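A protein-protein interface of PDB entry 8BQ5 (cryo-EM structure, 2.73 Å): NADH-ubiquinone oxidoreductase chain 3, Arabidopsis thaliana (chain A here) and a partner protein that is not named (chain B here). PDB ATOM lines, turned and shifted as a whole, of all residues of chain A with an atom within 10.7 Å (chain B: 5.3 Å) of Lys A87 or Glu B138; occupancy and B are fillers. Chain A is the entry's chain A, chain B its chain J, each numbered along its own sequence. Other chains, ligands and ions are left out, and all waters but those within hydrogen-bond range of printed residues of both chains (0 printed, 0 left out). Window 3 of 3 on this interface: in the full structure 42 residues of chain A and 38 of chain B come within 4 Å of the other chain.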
ATOM      1  N   FME A   1      35.583 -13.052  21.760  1.00  0.00           N
ATOM      2  CN  FME A   1      34.438 -13.256  21.020  1.00  0.00           C
ATOM      3  O1  FME A   1      34.416 -13.322  19.781  1.00  0.00           O
ATOM      4  CA  FME A   1      36.887 -12.907  21.177  1.00  0.00           C
ATOM      5  CB  FME A   1      37.947 -12.348  22.152  1.00  0.00           C
ATOM      6  CG  FME A   1      37.497 -11.116  22.893  1.00  0.00           C
ATOM      7  SD  FME A   1      37.137  -9.844  21.712  1.00  0.00           S
ATOM      8  CE  FME A   1      38.693  -9.084  21.458  1.00  0.00           C
ATOM      9  C   FME A   1      37.434 -14.235  20.660  1.00  0.00           C
ATOM     10  O   FME A   1      37.131 -15.329  21.410  1.00  0.00           O
ATOM     11  N   THR A  76      24.150 -31.550  18.525  1.00  0.00           N
ATOM     12  CA  THR A  76      24.333 -30.174  17.995  1.00  0.00           C
ATOM     13  C   THR A  76      23.230 -29.252  18.516  1.00  0.00           C
ATOM     14  O   THR A  76      23.579 -28.202  19.048  1.00  0.00           O
ATOM     15  CB  THR A  76      24.324 -30.179  16.461  1.00  0.00           C
ATOM     16  OG1 THR A  76      25.470 -30.906  16.016  1.00  0.00           O
ATOM     17  CG2 THR A  76      24.315 -28.796  15.848  1.00  0.00           C
ATOM     18  N   PHE A  77      21.961 -29.648  18.380  1.00  0.00           N
ATOM     19  CA  PHE A  77      20.809 -28.800  18.800  1.00  0.00           C
ATOM     20  C   PHE A  77      20.712 -28.721  20.331  1.00  0.00           C
ATOM     21  O   PHE A  77      20.053 -27.825  20.818  1.00  0.00           O
ATOM     22  CB  PHE A  77      19.520 -29.312  18.158  1.00  0.00           C
ATOM     23  CG  PHE A  77      19.292 -28.877  16.733  1.00  0.00           C
ATOM     24  CD1 PHE A  77      18.916 -27.575  16.441  1.00  0.00           C
ATOM     25  CD2 PHE A  77      19.436 -29.769  15.684  1.00  0.00           C
ATOM     26  CE1 PHE A  77      18.693 -27.177  15.133  1.00  0.00           C
ATOM     27  CE2 PHE A  77      19.220 -29.368  14.376  1.00  0.00           C
ATOM     28  CZ  PHE A  77      18.850 -28.073  14.102  1.00  0.00           C
ATOM     29  N   PHE A  78      21.331 -29.643  21.059  1.00  0.00           N
ATOM     30  CA  PHE A  78      21.344 -29.589  22.545  1.00  0.00           C
ATOM     31  C   PHE A  78      22.289 -28.504  23.077  1.00  0.00           C
ATOM     32  O   PHE A  78      21.968 -27.952  24.123  1.00  0.00           O
ATOM     33  CB  PHE A  78      21.778 -30.927  23.145  1.00  0.00           C
ATOM     34  CG  PHE A  78      20.673 -31.902  23.445  1.00  0.00           C
ATOM     35  CD1 PHE A  78      19.551 -31.504  24.152  1.00  0.00           C
ATOM     36  CD2 PHE A  78      20.772 -33.226  23.053  1.00  0.00           C
ATOM     37  CE1 PHE A  78      18.539 -32.405  24.440  1.00  0.00           C
ATOM     38  CE2 PHE A  78      19.759 -34.126  23.341  1.00  0.00           C
ATOM     39  CZ  PHE A  78      18.648 -33.713  24.036  1.00  0.00           C
ATOM     40  N   PHE A  79      23.421 -28.248  22.417  1.00  0.00           N
ATOM     41  CA  PHE A  79      24.432 -27.290  22.948  1.00  0.00           C
ATOM     42  C   PHE A  79      23.830 -25.884  23.113  1.00  0.00           C
ATOM     43  O   PHE A  79      23.964 -25.357  24.223  1.00  0.00           O
ATOM     44  CB  PHE A  79      25.701 -27.260  22.083  1.00  0.00           C
ATOM     45  CG  PHE A  79      26.793 -28.233  22.445  1.00  0.00           C
ATOM     46  CD1 PHE A  79      26.791 -29.527  21.948  1.00  0.00           C
ATOM     47  CD2 PHE A  79      27.855 -27.841  23.243  1.00  0.00           C
ATOM     48  CE1 PHE A  79      27.802 -30.414  22.280  1.00  0.00           C
ATOM     49  CE2 PHE A  79      28.866 -28.729  23.573  1.00  0.00           C
ATOM     50  CZ  PHE A  79      28.838 -30.015  23.093  1.00  0.00           C
ATOM     51  N   PRO A  80      23.180 -25.246  22.109  1.00  0.00           N
ATOM     52  CA  PRO A  80      22.590 -23.926  22.325  1.00  0.00           C
ATOM     53  C   PRO A  80      21.508 -24.020  23.405  1.00  0.00           C
ATOM     54  O   PRO A  80      21.452 -23.147  24.221  1.00  0.00           O
ATOM     55  CB  PRO A  80      21.987 -23.550  20.960  1.00  0.00           C
ATOM     56  CG  PRO A  80      22.680 -24.443  19.967  1.00  0.00           C
ATOM     57  CD  PRO A  80      22.974 -25.709  20.737  1.00  0.00           C
ATOM     58  N   TRP A  81      20.708 -25.087  23.396  1.00  0.00           N
ATOM     59  CA  TRP A  81      19.599 -25.278  24.365  1.00  0.00           C
ATOM     60  C   TRP A  81      20.137 -25.373  25.782  1.00  0.00           C
ATOM     61  O   TRP A  81      19.568 -24.731  26.663  1.00  0.00           O
ATOM     62  CB  TRP A  81      18.839 -26.555  23.993  1.00  0.00           C
ATOM     63  CG  TRP A  81      17.688 -26.896  24.885  1.00  0.00           C
ATOM     64  CD1 TRP A  81      16.468 -26.291  24.925  1.00  0.00           C
ATOM     65  CD2 TRP A  81      17.638 -27.963  25.846  1.00  0.00           C
ATOM     66  NE1 TRP A  81      15.670 -26.892  25.858  1.00  0.00           N
ATOM     67  CE2 TRP A  81      16.358 -27.924  26.436  1.00  0.00           C
ATOM     68  CE3 TRP A  81      18.549 -28.934  26.270  1.00  0.00           C
ATOM     69  CZ2 TRP A  81      15.969 -28.826  27.423  1.00  0.00           C
ATOM     70  CZ3 TRP A  81      18.161 -29.826  27.242  1.00  0.00           C
ATOM     71  CH2 TRP A  81      16.890 -29.769  27.810  1.00  0.00           C
ATOM     72  N   ALA A  82      21.168 -26.188  25.977  1.00  0.00           N
ATOM     73  CA  ALA A  82      21.728 -26.421  27.321  1.00  0.00           C
ATOM     74  C   ALA A  82      22.309 -25.119  27.858  1.00  0.00           C
ATOM     75  O   ALA A  82      22.072 -24.821  29.029  1.00  0.00           O
ATOM     76  CB  ALA A  82      22.779 -27.495  27.248  1.00  0.00           C
ATOM     77  N   VAL A  83      23.029 -24.371  27.022  1.00  0.00           N
ATOM     78  CA  VAL A  83      23.526 -23.114  27.587  1.00  0.00           C
ATOM     79  C   VAL A  83      22.446 -22.051  27.718  1.00  0.00           C
ATOM     80  O   VAL A  83      22.659 -21.055  28.420  1.00  0.00           O
ATOM     81  CB  VAL A  83      24.701 -22.533  26.780  1.00  0.00           C
ATOM     82  CG1 VAL A  83      25.878 -23.495  26.794  1.00  0.00           C
ATOM     83  CG2 VAL A  83      24.276 -22.212  25.363  1.00  0.00           C
ATOM     84  N   SER A  84      21.286 -22.232  27.086  1.00  0.00           N
ATOM     85  CA  SER A  84      20.249 -21.209  27.078  1.00  0.00           C
ATOM     86  C   SER A  84      19.033 -21.547  27.929  1.00  0.00           C
ATOM     87  O   SER A  84      18.051 -20.801  27.889  1.00  0.00           O
ATOM     88  CB  SER A  84      19.791 -20.945  25.641  1.00  0.00           C
ATOM     89  OG  SER A  84      20.869 -20.510  24.835  1.00  0.00           O
ATOM     90  N   LEU A  85      19.062 -22.646  28.687  1.00  0.00           N
ATOM     91  CA  LEU A  85      17.898 -23.018  29.491  1.00  0.00           C
ATOM     92  C   LEU A  85      17.473 -21.914  30.455  1.00  0.00           C
ATOM     93  O   LEU A  85      16.291 -21.814  30.800  1.00  0.00           O
ATOM     94  CB  LEU A  85      18.186 -24.298  30.271  1.00  0.00           C
ATOM     95  CG  LEU A  85      17.716 -25.616  29.663  1.00  0.00           C
ATOM     96  CD1 LEU A  85      17.966 -26.741  30.647  1.00  0.00           C
ATOM     97  CD2 LEU A  85      16.249 -25.548  29.279  1.00  0.00           C
ATOM     98  N   ASN A  86      18.415 -21.080  30.904  1.00  0.00           N
ATOM     99  CA  ASN A  86      18.101 -20.058  31.897  1.00  0.00           C
ATOM    100  C   ASN A  86      17.194 -18.958  31.357  1.00  0.00           C
ATOM    101  O   ASN A  86      16.553 -18.262  32.149  1.00  0.00           O
ATOM    102  CB  ASN A  86      19.392 -19.446  32.447  1.00  0.00           C
ATOM    103  CG  ASN A  86      20.159 -18.650  31.402  1.00  0.00           C
ATOM    104  OD1 ASN A  86      20.367 -19.110  30.281  1.00  0.00           O
ATOM    105  ND2 ASN A  86      20.589 -17.450  31.775  1.00  0.00           N
ATOM    106  N   LYS A  87      17.117 -18.783  30.039  1.00  0.00           N
ATOM    107  CA  LYS A  87      16.323 -17.704  29.465  1.00  0.00           C
ATOM    108  C   LYS A  87      15.095 -18.182  28.703  1.00  0.00           C
ATOM    109  O   LYS A  87      14.113 -17.439  28.616  1.00  0.00           O
ATOM    110  CB  LYS A  87      17.185 -16.851  28.536  1.00  0.00           C
ATOM    111  CG  LYS A  87      18.399 -16.249  29.215  1.00  0.00           C
ATOM    112  CD  LYS A  87      19.467 -15.879  28.212  1.00  0.00           C
ATOM    113  CE  LYS A  87      19.494 -16.864  27.070  1.00  0.00           C
ATOM    114  NZ  LYS A  87      20.876 -17.043  26.548  1.00  0.00           N
ATOM    115  N   ILE A  88      15.124 -19.393  28.144  1.00  0.00           N
ATOM    116  CA  ILE A  88      13.962 -19.900  27.420  1.00  0.00           C
ATOM    117  C   ILE A  88      12.904 -20.470  28.355  1.00  0.00           C
ATOM    118  O   ILE A  88      11.733 -20.559  27.968  1.00  0.00           O
ATOM    119  CB  ILE A  88      14.387 -20.954  26.386  1.00  0.00           C
ATOM    120  CG1 ILE A  88      14.975 -22.184  27.082  1.00  0.00           C
ATOM    121  CG2 ILE A  88      15.373 -20.352  25.399  1.00  0.00           C
ATOM    122  CD1 ILE A  88      15.729 -23.107  26.161  1.00  0.00           C
ATOM    123  N   ASP A  89      13.292 -20.868  29.561  1.00  0.00           N
ATOM    124  CA  ASP A  89      12.387 -21.277  30.651  1.00  0.00           C
ATOM    125  C   ASP A  89      11.539 -22.465  30.178  1.00  0.00           C
ATOM    126  O   ASP A  89      12.072 -23.399  29.561  1.00  0.00           O
ATOM    127  CB  ASP A  89      11.598 -20.080  31.125  1.00  0.00           C
ATOM    128  CG  ASP A  89      11.206 -20.189  32.585  1.00  0.00           C
ATOM    129  OD1 ASP A  89      11.370 -21.285  33.161  1.00  0.00           O
ATOM    130  OD2 ASP A  89      10.741 -19.182  33.157  1.00  0.00           O
ATOM    131  N   LEU A  90      10.233 -22.462  30.458  1.00  0.00           N
ATOM    132  CA  LEU A  90       9.403 -23.639  30.214  1.00  0.00           C
ATOM    133  C   LEU A  90       9.153 -23.859  28.728  1.00  0.00           C
ATOM    134  O   LEU A  90       9.091 -25.004  28.269  1.00  0.00           O
ATOM    135  CB  LEU A  90       8.076 -23.502  30.955  1.00  0.00           C
ATOM    136  CG  LEU A  90       8.031 -23.882  32.432  1.00  0.00           C
ATOM    137  CD1 LEU A  90       6.602 -23.780  32.930  1.00  0.00           C
ATOM    138  CD2 LEU A  90       8.590 -25.279  32.655  1.00  0.00           C
ATOM    139  N   PHE A  91       8.981 -22.777  27.967  1.00  0.00           N
ATOM    140  CA  PHE A  91       8.657 -22.905  26.550  1.00  0.00           C
ATOM    141  C   PHE A  91       9.767 -23.617  25.789  1.00  0.00           C
ATOM    142  O   PHE A  91       9.506 -24.543  25.011  1.00  0.00           O
ATOM    143  CB  PHE A  91       8.398 -21.524  25.947  1.00  0.00           C
ATOM    144  CG  PHE A  91       7.675 -21.558  24.633  1.00  0.00           C
ATOM    145  CD1 PHE A  91       8.334 -21.925  23.471  1.00  0.00           C
ATOM    146  CD2 PHE A  91       6.337 -21.215  24.557  1.00  0.00           C
ATOM    147  CE1 PHE A  91       7.673 -21.955  22.264  1.00  0.00           C
ATOM    148  CE2 PHE A  91       5.672 -21.242  23.350  1.00  0.00           C
ATOM    149  CZ  PHE A  91       6.340 -21.613  22.203  1.00  0.00           C
ATOM    150  N   GLY A  92      11.015 -23.186  25.986  1.00  0.00           N
ATOM    151  CA  GLY A  92      12.122 -23.823  25.291  1.00  0.00           C
ATOM    152  C   GLY A  92      12.315 -25.264  25.716  1.00  0.00           C
ATOM    153  O   GLY A  92      12.635 -26.131  24.894  1.00  0.00           O
ATOM    154  N   PHE A  93      12.108 -25.540  27.003  1.00  0.00           N
ATOM    155  CA  PHE A  93      12.200 -26.908  27.498  1.00  0.00           C
ATOM    156  C   PHE A  93      11.224 -27.819  26.763  1.00  0.00           C
ATOM    157  O   PHE A  93      11.597 -28.899  26.294  1.00  0.00           O
ATOM    158  CB  PHE A  93      11.945 -26.929  29.006  1.00  0.00           C
ATOM    159  CG  PHE A  93      11.916 -28.305  29.594  1.00  0.00           C
ATOM    160  CD1 PHE A  93      13.090 -28.938  29.960  1.00  0.00           C
ATOM    161  CD2 PHE A  93      10.716 -28.968  29.781  1.00  0.00           C
ATOM    162  CE1 PHE A  93      13.070 -30.206  30.497  1.00  0.00           C
ATOM    163  CE2 PHE A  93      10.691 -30.238  30.315  1.00  0.00           C
ATOM    164  CZ  PHE A  93      11.868 -30.857  30.676  1.00  0.00           C
ATOM    165  N   SER A  95       9.621 -27.242  23.839  1.00  0.00           N
ATOM    166  CA  SER A  95       9.918 -27.332  22.413  1.00  0.00           C
ATOM    167  C   SER A  95      11.020 -28.354  22.152  1.00  0.00           C
ATOM    168  O   SER A  95      10.919 -29.173  21.225  1.00  0.00           O
ATOM    169  CB  SER A  95      10.301 -25.957  21.865  1.00  0.00           C
ATOM    170  OG  SER A  95      11.549 -25.527  22.375  1.00  0.00           O
ATOM    171  N   SER B 133      28.779  -9.831  27.628  1.00  0.00           N
ATOM    172  CA  SER B 133      28.857 -10.294  26.252  1.00  0.00           C
ATOM    173  C   SER B 133      28.181 -11.650  26.094  1.00  0.00           C
ATOM    174  O   SER B 133      28.318 -12.534  26.944  1.00  0.00           O
ATOM    175  CB  SER B 133      30.314 -10.377  25.805  1.00  0.00           C
ATOM    176  OG  SER B 133      31.130 -10.921  26.828  1.00  0.00           O
ATOM    177  N   TRP B 134      27.438 -11.801  25.001  1.00  0.00           N
ATOM    178  CA  TRP B 134      26.822 -13.065  24.627  1.00  0.00           C
ATOM    179  C   TRP B 134      27.726 -13.795  23.645  1.00  0.00           C
ATOM    180  O   TRP B 134      28.265 -13.187  22.717  1.00  0.00           O
ATOM    181  CB  TRP B 134      25.452 -12.845  23.981  1.00  0.00           C
ATOM    182  CG  TRP B 134      24.318 -12.637  24.938  1.00  0.00           C
ATOM    183  CD1 TRP B 134      24.400 -12.218  26.232  1.00  0.00           C
ATOM    184  CD2 TRP B 134      22.922 -12.814  24.662  1.00  0.00           C
ATOM    185  NE1 TRP B 134      23.145 -12.135  26.784  1.00  0.00           N
ATOM    186  CE2 TRP B 134      22.219 -12.494  25.839  1.00  0.00           C
ATOM    187  CE3 TRP B 134      22.198 -13.218  23.535  1.00  0.00           C
ATOM    188  CZ2 TRP B 134      20.831 -12.563  25.922  1.00  0.00           C
ATOM    189  CZ3 TRP B 134      20.819 -13.285  23.620  1.00  0.00           C
ATOM    190  CH2 TRP B 134      20.151 -12.961  24.804  1.00  0.00           C
ATOM    191  N   THR B 135      27.892 -15.097  23.848  1.00  0.00           N
ATOM    192  CA  THR B 135      28.567 -15.887  22.834  1.00  0.00           C
ATOM    193  C   THR B 135      27.621 -16.142  21.664  1.00  0.00           C
ATOM    194  O   THR B 135      26.405 -15.960  21.762  1.00  0.00           O
ATOM    195  CB  THR B 135      29.070 -17.211  23.412  1.00  0.00           C
ATOM    196  OG1 THR B 135      27.971 -18.106  23.609  1.00  0.00           O
ATOM    197  CG2 THR B 135      29.775 -16.981  24.737  1.00  0.00           C
ATOM    198  N   ASN B 136      28.200 -16.548  20.534  1.00  0.00           N
ATOM    199  CA  ASN B 136      27.388 -16.894  19.374  1.00  0.00           C
ATOM    200  C   ASN B 136      26.450 -18.051  19.713  1.00  0.00           C
ATOM    201  O   ASN B 136      25.305 -18.107  19.237  1.00  0.00           O
ATOM    202  CB  ASN B 136      28.319 -17.212  18.195  1.00  0.00           C
ATOM    203  CG  ASN B 136      27.657 -18.029  17.107  1.00  0.00           C
ATOM    204  OD1 ASN B 136      26.555 -17.722  16.664  1.00  0.00           O
ATOM    205  ND2 ASN B 136      28.360 -19.045  16.629  1.00  0.00           N
ATOM    206  N   LEU B 137      26.903 -18.939  20.602  1.00  0.00           N
ATOM    207  CA  LEU B 137      26.080 -20.046  21.079  1.00  0.00           C
ATOM    208  C   LEU B 137      24.844 -19.546  21.821  1.00  0.00           C
ATOM    209  O   LEU B 137      23.722 -19.984  21.542  1.00  0.00           O
ATOM    210  CB  LEU B 137      26.919 -20.954  21.979  1.00  0.00           C
ATOM    211  CG  LEU B 137      26.337 -22.313  22.363  1.00  0.00           C
ATOM    212  CD1 LEU B 137      25.767 -22.992  21.144  1.00  0.00           C
ATOM    213  CD2 LEU B 137      27.388 -23.186  23.021  1.00  0.00           C
ATOM    214  N   GLU B 138      25.030 -18.636  22.785  1.00  0.00           N
ATOM    215  CA  GLU B 138      23.877 -18.126  23.522  1.00  0.00           C
ATOM    216  C   GLU B 138      22.946 -17.309  22.641  1.00  0.00           C
ATOM    217  O   GLU B 138      21.727 -17.369  22.823  1.00  0.00           O
ATOM    218  CB  GLU B 138      24.292 -17.267  24.717  1.00  0.00           C
ATOM    219  CG  GLU B 138      25.506 -17.712  25.487  1.00  0.00           C
ATOM    220  CD  GLU B 138      25.990 -16.623  26.424  1.00  0.00           C
ATOM    221  OE1 GLU B 138      27.213 -16.499  26.628  1.00  0.00           O
ATOM    222  OE2 GLU B 138      25.134 -15.880  26.949  1.00  0.00           O
ATOM    223  N   THR B 139      23.487 -16.532  21.704  1.00  0.00           N
ATOM    224  CA  THR B 139      22.620 -15.758  20.825  1.00  0.00           C
ATOM    225  C   THR B 139      21.752 -16.672  19.968  1.00  0.00           C
ATOM    226  O   THR B 139      20.558 -16.409  19.785  1.00  0.00           O
ATOM    227  CB  THR B 139      23.450 -14.810  19.957  1.00  0.00           C
ATOM    228  OG1 THR B 139      24.398 -14.119  20.777  1.00  0.00           O
ATOM    229  CG2 THR B 139      22.549 -13.784  19.302  1.00  0.00           C
ATOM    230  N   LEU B 140      22.325 -17.764  19.446  1.00  0.00           N
ATOM    231  CA  LEU B 140      21.515 -18.713  18.679  1.00  0.00           C
ATOM    232  C   LEU B 140      20.492 -19.429  19.562  1.00  0.00           C
ATOM    233  O   LEU B 140      19.325 -19.601  19.170  1.00  0.00           O
ATOM    234  CB  LEU B 140      22.422 -19.728  17.984  1.00  0.00           C
ATOM    235  CG  LEU B 140      21.824 -20.494  16.803  1.00  0.00           C
ATOM    236  CD1 LEU B 140      20.980 -19.576  15.935  1.00  0.00           C
ATOM    237  CD2 LEU B 140      22.929 -21.140  15.988  1.00  0.00           C
ATOM    238  N   GLY B 141      20.913 -19.856  20.757  1.00  0.00           N
ATOM    239  CA  GLY B 141      20.029 -20.583  21.648  1.00  0.00           C
ATOM    240  C   GLY B 141      18.918 -19.741  22.231  1.00  0.00           C
ATOM    241  O   GLY B 141      17.909 -20.291  22.682  1.00  0.00           O
ATOM    242  N   ASN B 142      19.087 -18.420  22.245  1.00  0.00           N
ATOM    243  CA  ASN B 142      18.010 -17.534  22.665  1.00  0.00           C
ATOM    244  C   ASN B 142      16.834 -17.559  21.696  1.00  0.00           C
ATOM    245  O   ASN B 142      15.708 -17.251  22.098  1.00  0.00           O
ATOM    246  CB  ASN B 142      18.542 -16.107  22.799  1.00  0.00           C
ATOM    247  CG  ASN B 142      17.480 -15.131  23.243  1.00  0.00           C
ATOM    248  OD1 ASN B 142      16.729 -15.400  24.178  1.00  0.00           O
ATOM    249  ND2 ASN B 142      17.399 -13.996  22.563  1.00  0.00           N
ATOM    250  N   LEU B 143      17.068 -17.927  20.437  1.00  0.00           N
ATOM    251  CA  LEU B 143      16.059 -17.832  19.391  1.00  0.00           C
ATOM    252  C   LEU B 143      15.528 -19.168  18.906  1.00  0.00           C
ATOM    253  O   LEU B 143      14.358 -19.240  18.522  1.00  0.00           O
ATOM    254  CB  LEU B 143      16.618 -17.084  18.178  1.00  0.00           C
ATOM    255  CG  LEU B 143      17.127 -15.670  18.416  1.00  0.00           C
ATOM    256  CD1 LEU B 143      17.778 -15.145  17.154  1.00  0.00           C
ATOM    257  CD2 LEU B 143      15.976 -14.792  18.840  1.00  0.00           C
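OG1 of Thr B135 sits at hydrogen-bond distance from N of Glu B138 (3.1 Å). The backbone carbonyl oxygen (O) of Pro A80 sits at hydrogen-bond distance from the side-chain hydroxyl (OG) of Ser A84 (2.8 Å). The backbone NH (N) of Leu B137 sits close to the side-chain hydroxyl (OG1) of Thr B135.
Among the printed residues, merely in contact across the chains: Phe A79 with Leu B137 (3.999 Å), Pro A80 with Leu B137 (3.5 Å), Pro A80 with Gly B141 (3.6 Å), Val A83 with Leu B137 (3.6 Å), Ser A84 with Glu B138 (3.8 Å), Ser A84 with Gly B141 (3.3 Å), Ser A84 with Asn B142 (3.8 Å), Lys A87 with Glu B138 (3.8 Å) and Ile A88 with Gly B141 (3.7 Å).
Of the 11 printed residues of chain B, 4 touch a printed residue of chain A. Hydrophobic or aromatic side chains of chain B within 4 Å of the printed part of chain A: Leu B137. Of the 20 printed residues of chain A, 6 touch a printed residue of chain B. Among the printed residues, no Asp or Glu carboxylate lies within 4 Å of a Lys or Arg side-chain nitrogen of the other chain.
Lys A87 touches just one residue of chain B: Glu B138 (3.8 Å). Glu B138 touches just these residues of chain A: Ser A84 and Lys A87. No residue of chain A comes within 4 Å of Trp B134. Gly B141 touches just these residues of chain A: Pro A80 (3.6 Å), Ser A84 (3.3 Å) and Ile A88 (3.7 Å). Printed residues of chain B within 4 Å of Ser A84: Glu B138, Gly B141 and Asn B142. Of the printed residues of chain B, Phe A79 touches Leu B137. Of the printed residues of chain B, Val A83 touches Leu B137 (3.6 Å). Printed residues of chain B within 4 Å of Ile A88: Gly B141. The nearest printed residue of chain B that does not touch Ile A88 is Asn B142 (4.5 Å).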
